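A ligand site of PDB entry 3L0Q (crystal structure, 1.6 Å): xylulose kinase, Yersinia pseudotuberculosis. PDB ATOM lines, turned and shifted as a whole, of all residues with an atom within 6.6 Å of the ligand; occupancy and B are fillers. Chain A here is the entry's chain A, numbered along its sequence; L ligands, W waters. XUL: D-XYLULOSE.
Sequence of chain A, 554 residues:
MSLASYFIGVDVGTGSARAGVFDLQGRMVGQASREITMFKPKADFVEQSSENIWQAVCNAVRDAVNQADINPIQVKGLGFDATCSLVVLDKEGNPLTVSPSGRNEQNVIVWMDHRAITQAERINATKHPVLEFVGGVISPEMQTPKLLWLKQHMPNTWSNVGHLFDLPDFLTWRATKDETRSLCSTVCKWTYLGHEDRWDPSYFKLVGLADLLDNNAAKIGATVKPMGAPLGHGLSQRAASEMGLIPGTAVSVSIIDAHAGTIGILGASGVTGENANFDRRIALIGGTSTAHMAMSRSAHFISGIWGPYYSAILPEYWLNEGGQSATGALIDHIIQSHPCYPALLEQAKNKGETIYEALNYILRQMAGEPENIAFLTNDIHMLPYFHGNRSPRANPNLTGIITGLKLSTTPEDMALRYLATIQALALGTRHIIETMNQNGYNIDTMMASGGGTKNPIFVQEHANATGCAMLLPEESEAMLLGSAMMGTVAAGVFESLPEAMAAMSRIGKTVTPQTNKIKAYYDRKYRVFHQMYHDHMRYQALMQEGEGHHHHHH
SG of Cys 84 lies within hydrogen-bond range of O4 of the ligand (3.2 Å). The backbone NH (N) of Cys 84 lies within hydrogen-bond range of an oxygen (O2) of the ligand, at 3.0 Å. The side-chain carboxylate of Asp 257 is in hydrogen-bond range of an oxygen (O1) of the ligand, at 2.8 Å. The side-chain hydroxyl (OG) of Ser 289 sits at hydrogen-bond distance from an oxygen (O1) of the ligand, 3.5 Å away. The side-chain amino group of Lys 189 sits at hydrogen-bond distance from an oxygen (O5) of the ligand (2.9 Å). An oxygen (O5) of the ligand sits at hydrogen-bond distance from the side-chain carboxylate (OE2) of Glu 321 (2.5 Å).
Merely in contact with the ligand: Thr 83, Trp 111, His 259, Arg 390, Ala 258 and Trp 306. Hydrophobic or aromatic side chains that line the ligand: Trp 111, Ala 258, His 259 and Trp 306. Of the 25 residues printed, 11 come within 4 Å of the ligand.
Water W1 lies within hydrogen-bond range of an oxygen (O4) of the ligand (2.8 Å), the side-chain carboxylate (OE1) of Glu 141 (2.9 Å) and the side-chain sulfur (SG) of Cys 84 (3.5 Å).
The backbone NH (N) of Glu 321 lies within hydrogen-bond range of the backbone carbonyl oxygen (O) of Trp 306 (3.0 Å). NH2 of Arg 390 lies within salt-bridge range of OE1 of Glu 141, 3.3 Å away. NE2 of His 259 is in hydrogen-bond range of SG of Cys 188 (3.7 Å). The side-chain hydroxyl (OG1) of Thr 83 sits at hydrogen-bond distance from the side-chain hydroxyl (OG) of Ser 85. O of Ala 82 is in hydrogen-bond range of N of Asp 257, at 2.8 Å. The side-chain hydroxyl of Ser 85 is in hydrogen-bond range of the backbone NH of Trp 111 (2.9 Å). NE1 of Trp 111 lies within hydrogen-bond range of OG1 of Thr 14. OE1 of Glu 321 sits at hydrogen-bond distance from NE2 of His 259.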
ATOM      1  N   GLY A  13      25.907  18.295   9.158  1.00  0.00           N
ATOM      2  CA  GLY A  13      24.887  17.276   9.173  1.00  0.00           C
ATOM      3  C   GLY A  13      25.539  15.914   9.184  1.00  0.00           C
ATOM      4  O   GLY A  13      26.723  15.756   9.512  1.00  0.00           O
ATOM      5  N   THR A  14      24.775  14.893   8.810  1.00  0.00           N
ATOM      6  CA  THR A  14      25.325  13.554   8.789  1.00  0.00           C
ATOM      7  C   THR A  14      26.336  13.343   7.679  1.00  0.00           C
ATOM      8  O   THR A  14      27.364  12.717   7.890  1.00  0.00           O
ATOM      9  CB  THR A  14      24.158  12.537   8.628  1.00  0.00           C
ATOM     10  OG1 THR A  14      23.285  12.709   9.746  1.00  0.00           O
ATOM     11  CG2 THR A  14      24.668  11.142   8.581  1.00  0.00           C
ATOM     12  N   ALA A  82      25.147  21.355  14.742  1.00  0.00           N
ATOM     13  CA  ALA A  82      25.641  20.064  14.269  1.00  0.00           C
ATOM     14  C   ALA A  82      24.739  18.962  14.771  1.00  0.00           C
ATOM     15  O   ALA A  82      23.903  19.164  15.684  1.00  0.00           O
ATOM     16  CB  ALA A  82      27.094  19.836  14.745  1.00  0.00           C
ATOM     17  N   THR A  83      24.894  17.782  14.181  1.00  0.00           N
ATOM     18  CA  THR A  83      24.237  16.608  14.731  1.00  0.00           C
ATOM     19  C   THR A  83      24.673  16.386  16.162  1.00  0.00           C
ATOM     20  O   THR A  83      25.777  16.805  16.563  1.00  0.00           O
ATOM     21  CB  THR A  83      24.589  15.332  13.931  1.00  0.00           C
ATOM     22  OG1 THR A  83      26.000  15.070  14.042  1.00  0.00           O
ATOM     23  CG2 THR A  83      24.253  15.507  12.428  1.00  0.00           C
ATOM     24  N   CYS A  84      23.846  15.682  16.932  1.00  0.00           N
ATOM     25  CA  CYS A  84      24.205  15.422  18.323  1.00  0.00           C
ATOM     26  C   CYS A  84      25.170  14.246  18.518  1.00  0.00           C
ATOM     27  O   CYS A  84      24.844  13.250  19.203  1.00  0.00           O
ATOM     28  CB  CYS A  84      22.929  15.238  19.163  1.00  0.00           C
ATOM     29  SG  CYS A  84      21.848  13.986  18.360  1.00  0.00           S
ATOM     30  N   SER A  85      26.328  14.352  17.875  1.00  0.00           N
ATOM     31  CA  SER A  85      27.321  13.296  17.846  1.00  0.00           C
ATOM     32  C   SER A  85      28.323  13.576  18.970  1.00  0.00           C
ATOM     33  O   SER A  85      28.337  14.672  19.538  1.00  0.00           O
ATOM     34  CB  SER A  85      27.991  13.279  16.473  1.00  0.00           C
ATOM     35  OG  SER A  85      27.040  12.879  15.474  1.00  0.00           O
ATOM     36  N   TRP A 111      25.596  10.400  15.965  1.00  0.00           N
ATOM     37  CA  TRP A 111      24.323  10.354  16.659  1.00  0.00           C
ATOM     38  C   TRP A 111      23.618   9.015  16.404  1.00  0.00           C
ATOM     39  O   TRP A 111      23.056   8.426  17.356  1.00  0.00           O
ATOM     40  CB  TRP A 111      23.442  11.523  16.188  1.00  0.00           C
ATOM     41  CG  TRP A 111      23.062  11.485  14.727  1.00  0.00           C
ATOM     42  CD1 TRP A 111      23.786  11.953  13.649  1.00  0.00           C
ATOM     43  CD2 TRP A 111      21.880  10.898  14.173  1.00  0.00           C
ATOM     44  NE1 TRP A 111      23.109  11.713  12.476  1.00  0.00           N
ATOM     45  CE2 TRP A 111      21.940  11.052  12.780  1.00  0.00           C
ATOM     46  CE3 TRP A 111      20.788  10.251  14.727  1.00  0.00           C
ATOM     47  CZ2 TRP A 111      20.919  10.602  11.949  1.00  0.00           C
ATOM     48  CZ3 TRP A 111      19.798   9.796  13.915  1.00  0.00           C
ATOM     49  CH2 TRP A 111      19.848   9.975  12.548  1.00  0.00           C
ATOM     50  N   MET A 112      23.664   8.538  15.159  1.00  0.00           N
ATOM     51  CA  MET A 112      22.833   7.368  14.736  1.00  0.00           C
ATOM     52  C   MET A 112      23.422   6.032  15.169  1.00  0.00           C
ATOM     53  O   MET A 112      22.818   4.970  14.960  1.00  0.00           O
ATOM     54  CB  MET A 112      22.607   7.368  13.203  1.00  0.00           C
ATOM     55  CG  MET A 112      23.942   7.405  12.448  1.00  0.00           C
ATOM     56  SD  MET A 112      23.644   7.227  10.520  1.00  0.00           S
ATOM     57  CE  MET A 112      22.205   8.515  10.174  1.00  0.00           C
ATOM     58  N   GLU A 141      21.029   6.510  21.347  1.00  0.00           N
ATOM     59  CA  GLU A 141      21.620   7.561  20.516  1.00  0.00           C
ATOM     60  C   GLU A 141      22.156   8.701  21.356  1.00  0.00           C
ATOM     61  O   GLU A 141      23.014   9.439  20.907  1.00  0.00           O
ATOM     62  CB  GLU A 141      20.628   8.033  19.437  1.00  0.00           C
ATOM     63  CG  GLU A 141      20.229   6.919  18.448  1.00  0.00           C
ATOM     64  CD  GLU A 141      19.178   7.340  17.415  1.00  0.00           C
ATOM     65  OE1 GLU A 141      18.816   8.547  17.324  1.00  0.00           O
ATOM     66  OE2 GLU A 141      18.707   6.432  16.679  1.00  0.00           O
ATOM     67  N   CYS A 188      19.403  18.407  26.383  1.00  0.00           N
ATOM     68  CA  CYS A 188      18.750  17.369  25.546  1.00  0.00           C
ATOM     69  C   CYS A 188      19.458  16.028  25.579  1.00  0.00           C
ATOM     70  O   CYS A 188      18.809  14.985  25.492  1.00  0.00           O
ATOM     71  CB  CYS A 188      18.628  17.824  24.080  1.00  0.00           C
ATOM     72  SG  CYS A 188      17.579  19.313  23.903  1.00  0.00           S
ATOM     73  N   LYS A 189      20.786  16.017  25.630  1.00  0.00           N
ATOM     74  CA  LYS A 189      21.496  14.770  25.387  1.00  0.00           C
ATOM     75  C   LYS A 189      22.417  14.272  26.474  1.00  0.00           C
ATOM     76  O   LYS A 189      22.945  13.171  26.355  1.00  0.00           O
ATOM     77  CB  LYS A 189      22.278  14.858  24.087  1.00  0.00           C
ATOM     78  CG  LYS A 189      21.500  15.500  22.958  1.00  0.00           C
ATOM     79  CD  LYS A 189      20.390  14.553  22.463  1.00  0.00           C
ATOM     80  CE  LYS A 189      19.809  15.099  21.175  1.00  0.00           C
ATOM     81  NZ  LYS A 189      18.717  14.209  20.687  1.00  0.00           N
ATOM     82  N   ILE A 256      22.017  22.202  18.593  1.00  0.00           N
ATOM     83  CA  ILE A 256      21.944  20.977  17.831  1.00  0.00           C
ATOM     84  C   ILE A 256      21.219  21.291  16.538  1.00  0.00           C
ATOM     85  O   ILE A 256      20.408  22.221  16.519  1.00  0.00           O
ATOM     86  CB  ILE A 256      21.190  19.896  18.648  1.00  0.00           C
ATOM     87  CG1 ILE A 256      22.112  19.420  19.776  1.00  0.00           C
ATOM     88  CG2 ILE A 256      20.784  18.704  17.756  1.00  0.00           C
ATOM     89  CD1 ILE A 256      21.368  18.591  20.741  1.00  0.00           C
ATOM     90  N   ASP A 257      21.493  20.536  15.459  1.00  0.00           N
ATOM     91  CA  ASP A 257      20.975  20.859  14.143  1.00  0.00           C
ATOM     92  C   ASP A 257      19.461  20.988  14.070  1.00  0.00           C
ATOM     93  O   ASP A 257      18.929  21.961  13.562  1.00  0.00           O
ATOM     94  CB  ASP A 257      21.512  19.874  13.039  1.00  0.00           C
ATOM     95  CG  ASP A 257      21.146  18.398  13.298  1.00  0.00           C
ATOM     96  OD1 ASP A 257      20.556  18.079  14.334  1.00  0.00           O
ATOM     97  OD2 ASP A 257      21.487  17.575  12.423  1.00  0.00           O
ATOM     98  N   ALA A 258      18.737  19.988  14.576  1.00  0.00           N
ATOM     99  CA  ALA A 258      17.293  20.037  14.485  1.00  0.00           C
ATOM    100  C   ALA A 258      16.751  21.276  15.181  1.00  0.00           C
ATOM    101  O   ALA A 258      15.824  21.925  14.683  1.00  0.00           O
ATOM    102  CB  ALA A 258      16.665  18.767  15.081  1.00  0.00           C
ATOM    103  N   HIS A 259      17.356  21.617  16.298  1.00  0.00           N
ATOM    104  CA  HIS A 259      16.983  22.832  17.049  1.00  0.00           C
ATOM    105  C   HIS A 259      17.297  24.171  16.353  1.00  0.00           C
ATOM    106  O   HIS A 259      16.588  25.163  16.512  1.00  0.00           O
ATOM    107  CB  HIS A 259      17.583  22.773  18.421  1.00  0.00           C
ATOM    108  CG  HIS A 259      17.369  21.432  19.074  1.00  0.00           C
ATOM    109  ND1 HIS A 259      17.894  20.264  18.571  1.00  0.00           N
ATOM    110  CD2 HIS A 259      16.673  21.101  20.191  1.00  0.00           C
ATOM    111  CE1 HIS A 259      17.554  19.262  19.371  1.00  0.00           C
ATOM    112  NE2 HIS A 259      16.799  19.746  20.351  1.00  0.00           N
ATOM    113  N   THR A 288      17.899  14.130   6.769  1.00  0.00           N
ATOM    114  CA  THR A 288      18.242  12.693   6.924  1.00  0.00           C
ATOM    115  C   THR A 288      17.253  12.002   7.847  1.00  0.00           C
ATOM    116  O   THR A 288      16.745  10.887   7.573  1.00  0.00           O
ATOM    117  CB  THR A 288      19.638  12.633   7.605  1.00  0.00           C
ATOM    118  OG1 THR A 288      20.556  13.361   6.782  1.00  0.00           O
ATOM    119  CG2 THR A 288      20.102  11.234   7.790  1.00  0.00           C
ATOM    120  N   SER A 289      17.051  12.678   8.972  1.00  0.00           N
ATOM    121  CA  SER A 289      16.054  12.377   9.992  1.00  0.00           C
ATOM    122  C   SER A 289      15.131  13.585  10.147  1.00  0.00           C
ATOM    123  O   SER A 289      15.391  14.671   9.564  1.00  0.00           O
ATOM    124  CB  SER A 289      16.797  11.989  11.293  1.00  0.00           C
ATOM    125  OG  SER A 289      17.561  13.072  11.809  1.00  0.00           O
ATOM    126  N   THR A 290      14.051  13.433  10.912  1.00  0.00           N
ATOM    127  CA  THR A 290      13.129  14.557  11.099  1.00  0.00           C
ATOM    128  C   THR A 290      12.851  14.739  12.567  1.00  0.00           C
ATOM    129  O   THR A 290      12.798  13.767  13.337  1.00  0.00           O
ATOM    130  CB  THR A 290      11.807  14.308  10.386  1.00  0.00           C
ATOM    131  OG1 THR A 290      12.078  14.240   9.005  1.00  0.00           O
ATOM    132  CG2 THR A 290      10.768  15.401  10.649  1.00  0.00           C
ATOM    133  N   ALA A 291      12.806  16.004  12.990  1.00  0.00           N
ATOM    134  CA  ALA A 291      12.453  16.323  14.361  1.00  0.00           C
ATOM    135  C   ALA A 291      11.065  16.972  14.381  1.00  0.00           C
ATOM    136  O   ALA A 291      10.668  17.669  13.433  1.00  0.00           O
ATOM    137  CB  ALA A 291      13.498  17.231  14.958  1.00  0.00           C
ATOM    138  N   MET A 293       8.983  19.364  16.724  1.00  0.00           N
ATOM    139  CA  MET A 293       9.309  20.228  17.883  1.00  0.00           C
ATOM    140  C   MET A 293       8.121  21.058  18.281  1.00  0.00           C
ATOM    141  O   MET A 293       7.596  21.832  17.454  1.00  0.00           O
ATOM    142  CB  MET A 293      10.429  21.163  17.507  1.00  0.00           C
ATOM    143  CG  MET A 293      11.527  20.575  16.701  1.00  0.00           C
ATOM    144  SD  MET A 293      12.466  19.527  17.989  1.00  0.00           S
ATOM    145  CE  MET A 293      13.678  20.823  18.177  1.00  0.00           C
ATOM    146  N   TRP A 306      10.920  12.824  23.754  1.00  0.00           N
ATOM    147  CA  TRP A 306      12.011  13.450  24.502  1.00  0.00           C
ATOM    148  C   TRP A 306      11.544  14.792  25.081  1.00  0.00           C
ATOM    149  O   TRP A 306      10.638  15.440  24.538  1.00  0.00           O
ATOM    150  CB  TRP A 306      13.274  13.632  23.607  1.00  0.00           C
ATOM    151  CG  TRP A 306      13.943  12.373  23.154  1.00  0.00           C
ATOM    152  CD1 TRP A 306      13.882  11.130  23.764  1.00  0.00           C
ATOM    153  CD2 TRP A 306      14.770  12.200  21.982  1.00  0.00           C
ATOM    154  NE1 TRP A 306      14.635  10.228  23.041  1.00  0.00           N
ATOM    155  CE2 TRP A 306      15.180  10.851  21.943  1.00  0.00           C
ATOM    156  CE3 TRP A 306      15.185  13.069  20.942  1.00  0.00           C
ATOM    157  CZ2 TRP A 306      16.015  10.347  20.953  1.00  0.00           C
ATOM    158  CZ3 TRP A 306      16.021  12.546  19.939  1.00  0.00           C
ATOM    159  CH2 TRP A 306      16.426  11.209  19.957  1.00  0.00           C
ATOM    160  N   GLU A 321      10.271  17.310  22.284  1.00  0.00           N
ATOM    161  CA  GLU A 321      10.960  16.962  21.021  1.00  0.00           C
ATOM    162  C   GLU A 321      10.668  15.529  20.571  1.00  0.00           C
ATOM    163  O   GLU A 321      11.201  14.558  21.142  1.00  0.00           O
ATOM    164  CB  GLU A 321      12.459  17.125  21.211  1.00  0.00           C
ATOM    165  CG  GLU A 321      13.182  16.713  19.918  1.00  0.00           C
ATOM    166  CD  GLU A 321      14.679  16.765  20.007  1.00  0.00           C
ATOM    167  OE1 GLU A 321      15.248  17.277  21.012  1.00  0.00           O
ATOM    168  OE2 GLU A 321      15.292  16.313  19.011  1.00  0.00           O
ATOM    169  N   GLY A 322       9.826  15.380  19.577  1.00  0.00           N
ATOM    170  CA  GLY A 322       9.621  14.094  18.917  1.00  0.00           C
ATOM    171  C   GLY A 322      10.614  13.958  17.764  1.00  0.00           C
ATOM    172  O   GLY A 322      11.285  14.919  17.338  1.00  0.00           O
ATOM    173  N   ARG A 390      11.935   6.304  17.246  1.00  0.00           N
ATOM    174  CA  ARG A 390      12.306   7.297  18.243  1.00  0.00           C
ATOM    175  C   ARG A 390      11.080   7.749  19.039  1.00  0.00           C
ATOM    176  O   ARG A 390      11.048   7.627  20.262  1.00  0.00           O
ATOM    177  CB  ARG A 390      12.978   8.501  17.581  1.00  0.00           C
ATOM    178  CG  ARG A 390      13.397   9.587  18.557  1.00  0.00           C
ATOM    179  CD  ARG A 390      14.016  10.777  17.829  1.00  0.00           C
ATOM    180  NE  ARG A 390      15.201  10.376  17.066  1.00  0.00           N
ATOM    181  CZ  ARG A 390      15.934  11.223  16.335  1.00  0.00           C
ATOM    182  NH1 ARG A 390      15.598  12.500  16.262  1.00  0.00           N
ATOM    183  NH2 ARG A 390      16.984  10.779  15.672  1.00  0.00           N
ATOM    184  N   MET A 479      18.181  25.247   8.931  1.00  0.00           N
ATOM    185  CA  MET A 479      19.223  25.045   9.946  1.00  0.00           C
ATOM    186  C   MET A 479      20.317  26.098   9.779  1.00  0.00           C
ATOM    187  O   MET A 479      20.778  26.748  10.740  1.00  0.00           O
ATOM    188  CB  MET A 479      19.748  23.613   9.916  1.00  0.00           C
ATOM    189  CG  MET A 479      18.578  22.587  10.000  1.00  0.00           C
ATOM    190  SD  MET A 479      19.431  20.877  10.059  1.00  0.00           S
ATOM    191  CE  MET A 479      17.887  19.844  10.498  1.00  0.00           C
HETATM  192  C1  XUL L   1      20.790  14.059  13.528  1.00  0.00           C
HETATM  193  C2  XUL L   1      20.585  14.596  14.935  1.00  0.00           C
HETATM  194  C3  XUL L   1      19.118  14.571  15.326  1.00  0.00           C
HETATM  195  C4  XUL L   1      18.990  14.823  16.818  1.00  0.00           C
HETATM  196  C5  XUL L   1      17.797  15.730  17.128  1.00  0.00           C
HETATM  197  O1  XUL L   1      20.308  15.046  12.609  1.00  0.00           O
HETATM  198  O2  XUL L   1      21.263  15.516  15.362  1.00  0.00           O
HETATM  199  O3  XUL L   1      18.515  15.648  14.625  1.00  0.00           O
HETATM  200  O4  XUL L   1      18.804  13.578  17.458  1.00  0.00           O
HETATM  201  O5  XUL L   1      17.673  15.885  18.532  1.00  0.00           O
HETATM  202  O   HOH W   1      19.864  11.092  18.096  1.00  0.00           O
